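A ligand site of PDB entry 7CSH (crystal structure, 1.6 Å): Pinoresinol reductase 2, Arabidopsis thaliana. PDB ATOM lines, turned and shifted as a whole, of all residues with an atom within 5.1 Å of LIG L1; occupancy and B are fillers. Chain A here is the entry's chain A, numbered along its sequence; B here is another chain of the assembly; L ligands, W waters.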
ATOM      1  N   GLY A  91      23.343  21.884 -16.033  1.00  0.00           N
ATOM      2  CA  GLY A  91      24.688  21.706 -16.541  1.00  0.00           C
ATOM      3  C   GLY A  91      24.756  21.933 -18.033  1.00  0.00           C
ATOM      4  O   GLY A  91      25.318  21.104 -18.759  1.00  0.00           O
ATOM      5  N   VAL A  92      24.173  23.036 -18.501  1.00  0.00           N
ATOM      6  CA  VAL A  92      24.175  23.401 -19.928  1.00  0.00           C
ATOM      7  C   VAL A  92      24.414  24.901 -19.994  1.00  0.00           C
ATOM      8  O   VAL A  92      23.656  25.661 -19.385  1.00  0.00           O
ATOM      9  CB  VAL A  92      22.849  23.053 -20.610  1.00  0.00           C
ATOM     10  CG1 VAL A  92      22.856  23.552 -22.069  1.00  0.00           C
ATOM     11  CG2 VAL A  92      22.596  21.553 -20.543  1.00  0.00           C
ATOM     12  N   PHE A  94      23.912  27.332 -22.092  1.00  0.00           N
ATOM     13  CA  PHE A  94      22.852  28.269 -22.488  1.00  0.00           C
ATOM     14  C   PHE A  94      21.614  28.225 -21.604  1.00  0.00           C
ATOM     15  O   PHE A  94      20.687  29.014 -21.829  1.00  0.00           O
ATOM     16  CB  PHE A  94      22.461  28.061 -23.968  1.00  0.00           C
ATOM     17  CG  PHE A  94      21.882  26.700 -24.313  1.00  0.00           C
ATOM     18  CD1 PHE A  94      20.586  26.325 -23.918  1.00  0.00           C
ATOM     19  CD2 PHE A  94      22.621  25.821 -25.090  1.00  0.00           C
ATOM     20  CE1 PHE A  94      20.088  25.068 -24.263  1.00  0.00           C
ATOM     21  CE2 PHE A  94      22.121  24.567 -25.455  1.00  0.00           C
ATOM     22  CZ  PHE A  94      20.863  24.194 -25.022  1.00  0.00           C
ATOM     23  N   GLY A 124      25.273  12.410 -19.329  1.00  0.00           N
ATOM     24  CA  GLY A 124      25.777  12.833 -20.622  1.00  0.00           C
ATOM     25  C   GLY A 124      27.125  12.198 -20.892  1.00  0.00           C
ATOM     26  O   GLY A 124      27.380  11.048 -20.487  1.00  0.00           O
ATOM     27  N   MET A 125      28.024  12.932 -21.552  1.00  0.00           N
ATOM     28  CA  MET A 125      29.388  12.424 -21.703  1.00  0.00           C
ATOM     29  C   MET A 125      29.989  12.107 -20.344  1.00  0.00           C
ATOM     30  O   MET A 125      29.797  12.836 -19.365  1.00  0.00           O
ATOM     31  CB  MET A 125      30.237  13.454 -22.449  1.00  0.00           C
ATOM     32  CG  MET A 125      29.902  13.521 -23.934  1.00  0.00           C
ATOM     33  SD  MET A 125      30.787  14.892 -24.754  1.00  0.00           S
ATOM     34  CE  MET A 125      29.730  16.256 -24.351  1.00  0.00           C
ATOM     35  N   THR A 140      32.019  21.798 -17.862  1.00  0.00           N
ATOM     36  CA  THR A 140      31.032  20.751 -17.585  1.00  0.00           C
ATOM     37  C   THR A 140      31.709  19.538 -16.967  1.00  0.00           C
ATOM     38  O   THR A 140      31.300  19.031 -15.916  1.00  0.00           O
ATOM     39  CB  THR A 140      30.300  20.380 -18.871  1.00  0.00           C
ATOM     40  OG1 THR A 140      29.660  21.553 -19.396  1.00  0.00           O
ATOM     41  CG2 THR A 140      29.250  19.286 -18.627  1.00  0.00           C
ATOM     42  N   PHE A 141      32.804  19.107 -17.585  1.00  0.00           N
ATOM     43  CA  PHE A 141      33.470  17.888 -17.129  1.00  0.00           C
ATOM     44  C   PHE A 141      34.279  18.136 -15.856  1.00  0.00           C
ATOM     45  O   PHE A 141      34.247  17.307 -14.939  1.00  0.00           O
ATOM     46  CB  PHE A 141      34.344  17.361 -18.270  1.00  0.00           C
ATOM     47  CG  PHE A 141      33.633  17.354 -19.597  1.00  0.00           C
ATOM     48  CD1 PHE A 141      32.386  16.742 -19.725  1.00  0.00           C
ATOM     49  CD2 PHE A 141      34.181  18.007 -20.688  1.00  0.00           C
ATOM     50  CE1 PHE A 141      31.716  16.770 -20.938  1.00  0.00           C
ATOM     51  CE2 PHE A 141      33.505  18.028 -21.902  1.00  0.00           C
ATOM     52  CZ  PHE A 141      32.287  17.402 -22.024  1.00  0.00           C
ATOM     53  N   LYS A 144      31.798  18.349 -12.961  1.00  0.00           N
ATOM     54  CA  LYS A 144      31.228  17.049 -12.589  1.00  0.00           C
ATOM     55  C   LYS A 144      32.267  16.164 -11.920  1.00  0.00           C
ATOM     56  O   LYS A 144      31.932  15.410 -11.010  1.00  0.00           O
ATOM     57  CB  LYS A 144      30.615  16.359 -13.817  1.00  0.00           C
ATOM     58  CG  LYS A 144      29.300  17.059 -14.280  1.00  0.00           C
ATOM     59  CD  LYS A 144      28.663  16.345 -15.449  1.00  0.00           C
ATOM     60  CE  LYS A 144      27.429  17.122 -15.927  1.00  0.00           C
ATOM     61  NZ  LYS A 144      26.713  16.395 -17.022  1.00  0.00           N
ATOM     62  N   ALA A 164      25.214   8.944 -23.537  1.00  0.00           N
ATOM     63  CA  ALA A 164      24.295   9.112 -24.651  1.00  0.00           C
ATOM     64  C   ALA A 164      23.878  10.570 -24.808  1.00  0.00           C
ATOM     65  O   ALA A 164      23.839  11.334 -23.835  1.00  0.00           O
ATOM     66  CB  ALA A 164      23.039   8.253 -24.459  1.00  0.00           C
ATOM     67  N   CYS A 165      23.578  10.940 -26.060  1.00  0.00           N
ATOM     68  CA  CYS A 165      22.987  12.231 -26.399  1.00  0.00           C
ATOM     69  C   CYS A 165      21.467  12.188 -26.234  1.00  0.00           C
ATOM     70  O   CYS A 165      20.830  11.259 -26.715  1.00  0.00           O
ATOM     71  CB  CYS A 165      23.299  12.572 -27.862  1.00  0.00           C
ATOM     72  SG  CYS A 165      24.992  13.029 -28.214  1.00  0.00           S
ATOM     73  N   TYR A 169      18.099  17.154 -28.226  1.00  0.00           N
ATOM     74  CA  TYR A 169      19.119  18.121 -28.588  1.00  0.00           C
ATOM     75  C   TYR A 169      19.964  17.679 -29.786  1.00  0.00           C
ATOM     76  O   TYR A 169      20.655  18.517 -30.385  1.00  0.00           O
ATOM     77  CB  TYR A 169      20.042  18.392 -27.391  1.00  0.00           C
ATOM     78  CG  TYR A 169      19.399  19.212 -26.285  1.00  0.00           C
ATOM     79  CD1 TYR A 169      19.090  20.548 -26.507  1.00  0.00           C
ATOM     80  CD2 TYR A 169      19.189  18.684 -25.029  1.00  0.00           C
ATOM     81  CE1 TYR A 169      18.528  21.330 -25.504  1.00  0.00           C
ATOM     82  CE2 TYR A 169      18.621  19.456 -24.006  1.00  0.00           C
ATOM     83  CZ  TYR A 169      18.319  20.774 -24.252  1.00  0.00           C
ATOM     84  OH  TYR A 169      17.778  21.549 -23.241  1.00  0.00           O
ATOM     85  N   PHE A 170      19.950  16.397 -30.120  1.00  0.00           N
ATOM     86  CA  PHE A 170      20.824  15.861 -31.152  1.00  0.00           C
ATOM     87  C   PHE A 170      20.097  15.028 -32.170  1.00  0.00           C
ATOM     88  O   PHE A 170      20.608  14.847 -33.286  1.00  0.00           O
ATOM     89  CB  PHE A 170      21.918  14.983 -30.516  1.00  0.00           C
ATOM     90  CG  PHE A 170      22.843  15.735 -29.575  1.00  0.00           C
ATOM     91  CD1 PHE A 170      23.970  16.381 -30.061  1.00  0.00           C
ATOM     92  CD2 PHE A 170      22.575  15.797 -28.210  1.00  0.00           C
ATOM     93  CE1 PHE A 170      24.831  17.035 -29.200  1.00  0.00           C
ATOM     94  CE2 PHE A 170      23.426  16.474 -27.365  1.00  0.00           C
ATOM     95  CZ  PHE A 170      24.540  17.105 -27.852  1.00  0.00           C
ATOM     96  N   ASN A 173      16.489  17.146 -34.268  1.00  0.00           N
ATOM     97  CA  ASN A 173      16.931  18.234 -35.127  1.00  0.00           C
ATOM     98  C   ASN A 173      17.979  17.783 -36.159  1.00  0.00           C
ATOM     99  O   ASN A 173      18.597  18.637 -36.791  1.00  0.00           O
ATOM    100  CB  ASN A 173      17.497  19.377 -34.276  1.00  0.00           C
ATOM    101  CG  ASN A 173      18.611  18.907 -33.340  1.00  0.00           C
ATOM    102  OD1 ASN A 173      19.023  17.741 -33.365  1.00  0.00           O
ATOM    103  ND2 ASN A 173      19.095  19.814 -32.507  1.00  0.00           N
ATOM    104  N   GLN A 176      21.420  19.545 -35.996  1.00  0.00           N
ATOM    105  CA  GLN A 176      21.684  20.915 -36.437  1.00  0.00           C
ATOM    106  C   GLN A 176      21.680  21.847 -35.230  1.00  0.00           C
ATOM    107  O   GLN A 176      20.757  21.806 -34.420  1.00  0.00           O
ATOM    108  CB  GLN A 176      20.623  21.368 -37.440  1.00  0.00           C
ATOM    109  CG  GLN A 176      20.491  20.451 -38.645  1.00  0.00           C
ATOM    110  CD  GLN A 176      21.796  20.303 -39.419  1.00  0.00           C
ATOM    111  OE1 GLN A 176      22.109  21.127 -40.276  1.00  0.00           O
ATOM    112  NE2 GLN A 176      22.557  19.252 -39.108  1.00  0.00           N
ATOM    113  N   MET A 177      22.710  22.675 -35.126  1.00  0.00           N
ATOM    114  CA  MET A 177      22.850  23.532 -33.951  1.00  0.00           C
ATOM    115  C   MET A 177      21.872  24.696 -34.017  1.00  0.00           C
ATOM    116  O   MET A 177      21.492  25.169 -35.107  1.00  0.00           O
ATOM    117  CB  MET A 177      24.278  24.073 -33.826  1.00  0.00           C
ATOM    118  CG  MET A 177      25.333  22.991 -33.612  1.00  0.00           C
ATOM    119  SD  MET A 177      26.980  23.658 -33.312  1.00  0.00           S
ATOM    120  CE  MET A 177      26.882  24.065 -31.566  1.00  0.00           C
ATOM    121  N   GLY A 178      21.464  25.158 -32.838  1.00  0.00           N
ATOM    122  CA  GLY A 178      20.673  26.369 -32.729  1.00  0.00           C
ATOM    123  C   GLY A 178      19.174  26.181 -32.890  1.00  0.00           C
ATOM    124  O   GLY A 178      18.430  27.169 -32.765  1.00  0.00           O
ATOM    125  N   THR A 179      18.714  24.966 -33.171  1.00  0.00           N
ATOM    126  CA  THR A 179      17.305  24.669 -33.344  1.00  0.00           C
ATOM    127  C   THR A 179      17.055  23.255 -32.839  1.00  0.00           C
ATOM    128  O   THR A 179      17.963  22.432 -32.830  1.00  0.00           O
ATOM    129  CB  THR A 179      16.890  24.782 -34.827  1.00  0.00           C
ATOM    130  OG1 THR A 179      15.489  24.517 -34.975  1.00  0.00           O
ATOM    131  CG2 THR A 179      17.707  23.809 -35.674  1.00  0.00           C
ATOM    132  N   LEU A 180      15.810  22.969 -32.455  1.00  0.00           N
ATOM    133  CA  LEU A 180      15.445  21.614 -32.045  1.00  0.00           C
ATOM    134  C   LEU A 180      14.496  20.971 -33.050  1.00  0.00           C
ATOM    135  O   LEU A 180      14.000  19.871 -32.806  1.00  0.00           O
ATOM    136  CB  LEU A 180      14.821  21.592 -30.645  1.00  0.00           C
ATOM    137  CG  LEU A 180      15.648  22.244 -29.539  1.00  0.00           C
ATOM    138  CD1 LEU A 180      14.981  22.072 -28.158  1.00  0.00           C
ATOM    139  CD2 LEU A 180      17.083  21.696 -29.499  1.00  0.00           C
ATOM    140  N   SER A 269      28.267  30.240 -24.627  1.00  0.00           N
ATOM    141  CA  SER A 269      27.467  29.021 -24.682  1.00  0.00           C
ATOM    142  C   SER A 269      27.590  28.343 -26.033  1.00  0.00           C
ATOM    143  O   SER A 269      27.469  27.114 -26.119  1.00  0.00           O
ATOM    144  CB  SER A 269      25.998  29.313 -24.351  1.00  0.00           C
ATOM    145  OG  SER A 269      25.347  30.031 -25.386  1.00  0.00           O
ATOM    146  N   HIS A 270      27.844  29.115 -27.086  1.00  0.00           N
ATOM    147  CA  HIS A 270      28.087  28.499 -28.387  1.00  0.00           C
ATOM    148  C   HIS A 270      29.459  27.839 -28.429  1.00  0.00           C
ATOM    149  O   HIS A 270      29.617  26.758 -29.010  1.00  0.00           O
ATOM    150  CB  HIS A 270      27.948  29.529 -29.506  1.00  0.00           C
ATOM    151  CG  HIS A 270      27.939  28.919 -30.868  1.00  0.00           C
ATOM    152  ND1 HIS A 270      26.955  28.046 -31.286  1.00  0.00           N
ATOM    153  CD2 HIS A 270      28.801  29.035 -31.907  1.00  0.00           C
ATOM    154  CE1 HIS A 270      27.212  27.672 -32.523  1.00  0.00           C
ATOM    155  NE2 HIS A 270      28.327  28.256 -32.926  1.00  0.00           N
ATOM    156  N   GLY A 273      28.998  24.537 -26.852  1.00  0.00           N
ATOM    157  CA  GLY A 273      28.324  23.634 -27.762  1.00  0.00           C
ATOM    158  C   GLY A 273      29.236  23.122 -28.854  1.00  0.00           C
ATOM    159  O   GLY A 273      29.242  21.928 -29.146  1.00  0.00           O
ATOM    160  N   HIS A 276      31.513  20.424 -27.369  1.00  0.00           N
ATOM    161  CA  HIS A 276      30.826  19.160 -27.135  1.00  0.00           C
ATOM    162  C   HIS A 276      30.541  18.448 -28.462  1.00  0.00           C
ATOM    163  O   HIS A 276      30.799  17.241 -28.592  1.00  0.00           O
ATOM    164  CB  HIS A 276      29.531  19.396 -26.369  1.00  0.00           C
ATOM    165  CG  HIS A 276      29.709  19.721 -24.918  1.00  0.00           C
ATOM    166  ND1 HIS A 276      30.907  20.143 -24.388  1.00  0.00           N
ATOM    167  CD2 HIS A 276      28.826  19.707 -23.893  1.00  0.00           C
ATOM    168  CE1 HIS A 276      30.753  20.392 -23.095  1.00  0.00           C
ATOM    169  NE2 HIS A 276      29.496  20.121 -22.769  1.00  0.00           N
ATOM    170  N   PHE A 277      29.973  19.167 -29.432  1.00  0.00           N
ATOM    171  CA  PHE A 277      29.718  18.576 -30.744  1.00  0.00           C
ATOM    172  C   PHE A 277      30.994  18.048 -31.378  1.00  0.00           C
ATOM    173  O   PHE A 277      30.974  17.015 -32.050  1.00  0.00           O
ATOM    174  CB  PHE A 277      29.066  19.587 -31.686  1.00  0.00           C
ATOM    175  CG  PHE A 277      27.550  19.641 -31.598  1.00  0.00           C
ATOM    176  CD1 PHE A 277      26.934  20.123 -30.461  1.00  0.00           C
ATOM    177  CD2 PHE A 277      26.762  19.236 -32.672  1.00  0.00           C
ATOM    178  CE1 PHE A 277      25.531  20.196 -30.379  1.00  0.00           C
ATOM    179  CE2 PHE A 277      25.359  19.297 -32.602  1.00  0.00           C
ATOM    180  CZ  PHE A 277      24.757  19.765 -31.468  1.00  0.00           C
ATOM    181  N   ILE A 280      31.772  14.675 -29.901  1.00  0.00           N
ATOM    182  CA  ILE A 280      30.794  13.654 -30.239  1.00  0.00           C
ATOM    183  C   ILE A 280      30.895  13.251 -31.711  1.00  0.00           C
ATOM    184  O   ILE A 280      30.949  12.055 -32.028  1.00  0.00           O
ATOM    185  CB  ILE A 280      29.379  14.155 -29.902  1.00  0.00           C
ATOM    186  CG1 ILE A 280      29.262  14.367 -28.395  1.00  0.00           C
ATOM    187  CG2 ILE A 280      28.337  13.167 -30.433  1.00  0.00           C
ATOM    188  CD1 ILE A 280      28.056  15.245 -28.039  1.00  0.00           C
ATOM    189  N   LEU A 286      31.554   9.051 -27.933  1.00  0.00           N
ATOM    190  CA  LEU A 286      30.568   8.181 -27.297  1.00  0.00           C
ATOM    191  C   LEU A 286      30.705   6.728 -27.738  1.00  0.00           C
ATOM    192  O   LEU A 286      30.065   5.856 -27.137  1.00  0.00           O
ATOM    193  CB  LEU A 286      29.148   8.667 -27.590  1.00  0.00           C
ATOM    194  CG  LEU A 286      28.789  10.044 -27.033  1.00  0.00           C
ATOM    195  CD1 LEU A 286      27.340  10.438 -27.398  1.00  0.00           C
ATOM    196  CD2 LEU A 286      28.979  10.080 -25.512  1.00  0.00           C
ATOM    197  N   VAL B  46      17.000  26.841 -28.859  1.00  0.00           N
ATOM    198  CA  VAL B  46      17.270  25.552 -28.232  1.00  0.00           C
ATOM    199  C   VAL B  46      16.527  25.414 -26.902  1.00  0.00           C
ATOM    200  O   VAL B  46      16.970  24.693 -26.004  1.00  0.00           O
ATOM    201  CB  VAL B  46      18.783  25.330 -28.050  1.00  0.00           C
ATOM    202  CG1 VAL B  46      19.454  25.132 -29.444  1.00  0.00           C
ATOM    203  CG2 VAL B  46      19.445  26.490 -27.335  1.00  0.00           C
HETATM  204  C1  LIG L   1      21.099  21.933 -30.730  1.00  0.00           C
HETATM  205  O1  LIG L   1      21.853  23.040 -30.606  1.00  0.00           O
HETATM  206  C2  LIG L   1      22.737  23.092 -29.640  1.00  0.00           C
HETATM  207  C3  LIG L   1      22.946  22.082 -28.736  1.00  0.00           C
HETATM  208  C4  LIG L   1      23.478  24.268 -29.547  1.00  0.00           C
HETATM  209  O2  LIG L   1      23.250  25.264 -30.411  1.00  0.00           O
HETATM  210  C5  LIG L   1      24.391  24.372 -28.535  1.00  0.00           C
HETATM  211  C6  LIG L   1      24.601  23.348 -27.633  1.00  0.00           C
HETATM  212  C7  LIG L   1      23.874  22.198 -27.704  1.00  0.00           C
HETATM  213  C8  LIG L   1      24.168  21.057 -26.805  1.00  0.00           C
HETATM  214  O3  LIG L   1      25.614  20.732 -26.967  1.00  0.00           O
HETATM  215  C9  LIG L   1      26.090  20.235 -25.827  1.00  0.00           C
HETATM  216  C10 LIG L   1      25.163  20.403 -24.692  1.00  0.00           C
HETATM  217  C11 LIG L   1      24.068  21.296 -25.335  1.00  0.00           C
HETATM  218  C12 LIG L   1      22.799  20.648 -24.728  1.00  0.00           C
HETATM  219  O4  LIG L   1      23.225  19.613 -23.792  1.00  0.00           O
HETATM  220  C13 LIG L   1      24.401  19.115 -24.314  1.00  0.00           C
HETATM  221  C14 LIG L   1      25.182  18.211 -23.487  1.00  0.00           C
HETATM  222  C15 LIG L   1      25.479  16.939 -23.944  1.00  0.00           C
HETATM  223  C16 LIG L   1      25.643  18.564 -22.245  1.00  0.00           C
HETATM  224  C17 LIG L   1      26.404  17.710 -21.470  1.00  0.00           C
HETATM  225  C18 LIG L   1      26.713  16.455 -21.946  1.00  0.00           C
HETATM  226  O5  LIG L   1      27.504  15.592 -21.255  1.00  0.00           O
HETATM  227  C19 LIG L   1      26.246  16.067 -23.192  1.00  0.00           C
HETATM  228  O6  LIG L   1      26.543  14.845 -23.611  1.00  0.00           O
HETATM  229  C20 LIG L   1      25.979  14.450 -24.832  1.00  0.00           C
HETATM  230  P1  LG2 L   2      18.022  22.251 -16.069  1.00  0.00           P
HETATM  231  O1  LG2 L   2      18.647  23.409 -16.678  1.00  0.00           O
HETATM  232  O2  LG2 L   2      16.664  22.016 -16.408  1.00  0.00           O
HETATM  233  O3  LG2 L   2      18.148  22.557 -14.454  1.00  0.00           O
HETATM  234  C1  LG2 L   2      17.866  21.476 -13.646  1.00  0.00           C
HETATM  235  C2  LG2 L   2      17.633  21.933 -12.187  1.00  0.00           C
HETATM  236  O4  LG2 L   2      18.737  22.539 -11.664  1.00  0.00           O
HETATM  237  C3  LG2 L   2      16.535  23.044 -12.069  1.00  0.00           C
HETATM  238  O5  LG2 L   2      15.233  22.692 -12.278  1.00  0.00           O
HETATM  239  C4  LG2 L   2      16.895  23.470 -10.576  1.00  0.00           C
HETATM  240  O6  LG2 L   2      16.064  22.683  -9.676  1.00  0.00           O
HETATM  241  C5  LG2 L   2      18.282  23.253 -10.364  1.00  0.00           C
HETATM  242  N1  LG2 L   2      19.172  24.429 -10.281  1.00  0.00           N
HETATM  243  C6  LG2 L   2      19.712  25.238 -11.167  1.00  0.00           C
HETATM  244  N2  LG2 L   2      20.386  26.190 -10.543  1.00  0.00           N
HETATM  245  C7  LG2 L   2      20.277  25.948  -9.254  1.00  0.00           C
HETATM  246  C8  LG2 L   2      20.834  26.578  -8.171  1.00  0.00           C
HETATM  247  N3  LG2 L   2      21.667  27.758  -8.185  1.00  0.00           N
HETATM  248  N4  LG2 L   2      20.610  26.134  -6.952  1.00  0.00           N
HETATM  249  C9  LG2 L   2      19.818  25.065  -6.764  1.00  0.00           C
HETATM  250  N5  LG2 L   2      19.292  24.431  -7.808  1.00  0.00           N
HETATM  251  C10 LG2 L   2      19.527  24.894  -9.056  1.00  0.00           C
HETATM  252  O7  LG2 L   2      18.973  20.925 -16.226  1.00  0.00           O
HETATM  253  P2  LG2 L   2      18.976  19.942 -17.481  1.00  0.00           P
HETATM  254  O8  LG2 L   2      17.936  18.967 -17.311  1.00  0.00           O
HETATM  255  O9  LG2 L   2      19.164  20.626 -18.734  1.00  0.00           O
HETATM  256  O10 LG2 L   2      20.345  19.178 -17.203  1.00  0.00           O
HETATM  257  C11 LG2 L   2      20.421  18.192 -16.256  1.00  0.00           C
HETATM  258  C12 LG2 L   2      21.664  17.247 -16.532  1.00  0.00           C
HETATM  259  O11 LG2 L   2      21.566  16.703 -17.687  1.00  0.00           O
HETATM  260  C13 LG2 L   2      23.055  18.031 -16.471  1.00  0.00           C
HETATM  261  O12 LG2 L   2      24.078  17.411 -15.854  1.00  0.00           O
HETATM  262  C14 LG2 L   2      23.398  18.117 -17.993  1.00  0.00           C
HETATM  263  O13 LG2 L   2      24.823  18.363 -18.254  1.00  0.00           O
HETATM  264  C15 LG2 L   2      22.917  16.907 -18.465  1.00  0.00           C
HETATM  265  N6  LG2 L   2      22.454  16.963 -19.861  1.00  0.00           N
HETATM  266  C16 LG2 L   2      22.827  16.026 -20.832  1.00  0.00           C
HETATM  267  C17 LG2 L   2      22.358  16.123 -22.172  1.00  0.00           C
HETATM  268  C18 LG2 L   2      22.651  14.974 -23.137  1.00  0.00           C
HETATM  269  O14 LG2 L   2      23.082  13.982 -22.632  1.00  0.00           O
HETATM  270  N7  LG2 L   2      22.394  15.206 -24.503  1.00  0.00           N
HETATM  271  C19 LG2 L   2      21.591  17.279 -22.710  1.00  0.00           C
HETATM  272  C20 LG2 L   2      21.318  18.333 -21.628  1.00  0.00           C
HETATM  273  C21 LG2 L   2      21.585  18.031 -20.172  1.00  0.00           C
HETATM  274  P3  LG2 L   2      14.592  22.966  -9.184  1.00  0.00           P
HETATM  275  O15 LG2 L   2      13.761  22.091  -9.988  1.00  0.00           O
HETATM  276  O16 LG2 L   2      14.532  22.616  -7.782  1.00  0.00           O
HETATM  277  O17 LG2 L   2      14.326  24.349  -9.474  1.00  0.00           O
HETATM  278  O   HOH W   1      27.322  21.185 -20.818  1.00  0.00           O
HETATM  279  O   HOH W   2      24.645  27.394 -30.016  1.00  0.00           O
HETATM  280  O   HOH W   3      28.632  15.594 -18.988  1.00  0.00           O
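An oxygen (O5) of LIG L1 lies within hydrogen-bond range of the backbone NH of Met 125. N of Gly 178 sits at hydrogen-bond distance from O2 of LIG L1, at 3.0 Å. The backbone carbonyl oxygen (O) of Gly 91 sits at hydrogen-bond distance from an oxygen (O13) of LG2 L2 (2.8 Å). NZ of Lys 144 is in hydrogen-bond range of O13 of LG2 L2 (3.0 Å).
O of Tyr 169 sits at hydrogen-bond distance from ND2 of Asn 173. ND2 of Asn 173 is in hydrogen-bond range of O of Gln 176. The side-chain amide nitrogen (ND2) of Asn 173 is in hydrogen-bond range of the backbone carbonyl oxygen (O) of Thr 179 (2.9 Å). OD1 of Asn 173 sits close to O of Phe 170, at 3.3 Å.
Merely in contact with LIG L1: Val 92 (3.8 Å), Phe 94 (3.5 Å), Gly 124 (3.3 Å), Ala 164 (3.9 Å), Cys 165 (3.8 Å), Tyr 169 (3.5 Å), Phe 170 (3.9 Å), Asn 173 (3.4 Å), Gln 176 (3.7 Å), Met 177 (3.5 Å), Thr 179 (3.8 Å), Gly 273 (3.7 Å), His 276 (3.4 Å), Phe 277 (3.5 Å), Ile 280 (3.9 Å) and Val 46 of chain B (3.4 Å). Hydrophobic or aromatic side chains within 4 Å of LIG L1: Val 92, Phe 94, Met 125, Phe 170, Met 177, His 276, Phe 277, Ile 280 and Val 46 of chain B. 18 residues have an atom within 4 Å of LIG L1: Val 92, Phe 94, Gly 124, Met 125, Ala 164, Cys 165, Tyr 169, Phe 170, Asn 173, Gln 176, Met 177, Gly 178, Thr 179, Gly 273, His 276, Phe 277, Ile 280 and Val 46 of chain B. The nearest printed residue that does not touch LIG L1 is Leu 180 (4.2 Å).
Water W3 lies within hydrogen-bond range of O5 of LIG L1 (2.5 Å), NZ of Lys 144 (2.9 Å) and O of Met 125 (3.0 Å). Water W2 lies within hydrogen-bond range of an oxygen (O2) of LIG L1 and a ring nitrogen (ND1) of His 270. Water W1 lies within hydrogen-bond range of the side-chain hydroxyl (OG1) of Thr 140, the backbone carbonyl oxygen (O) of Gly 91 and a ring nitrogen (NE2) of His 276.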
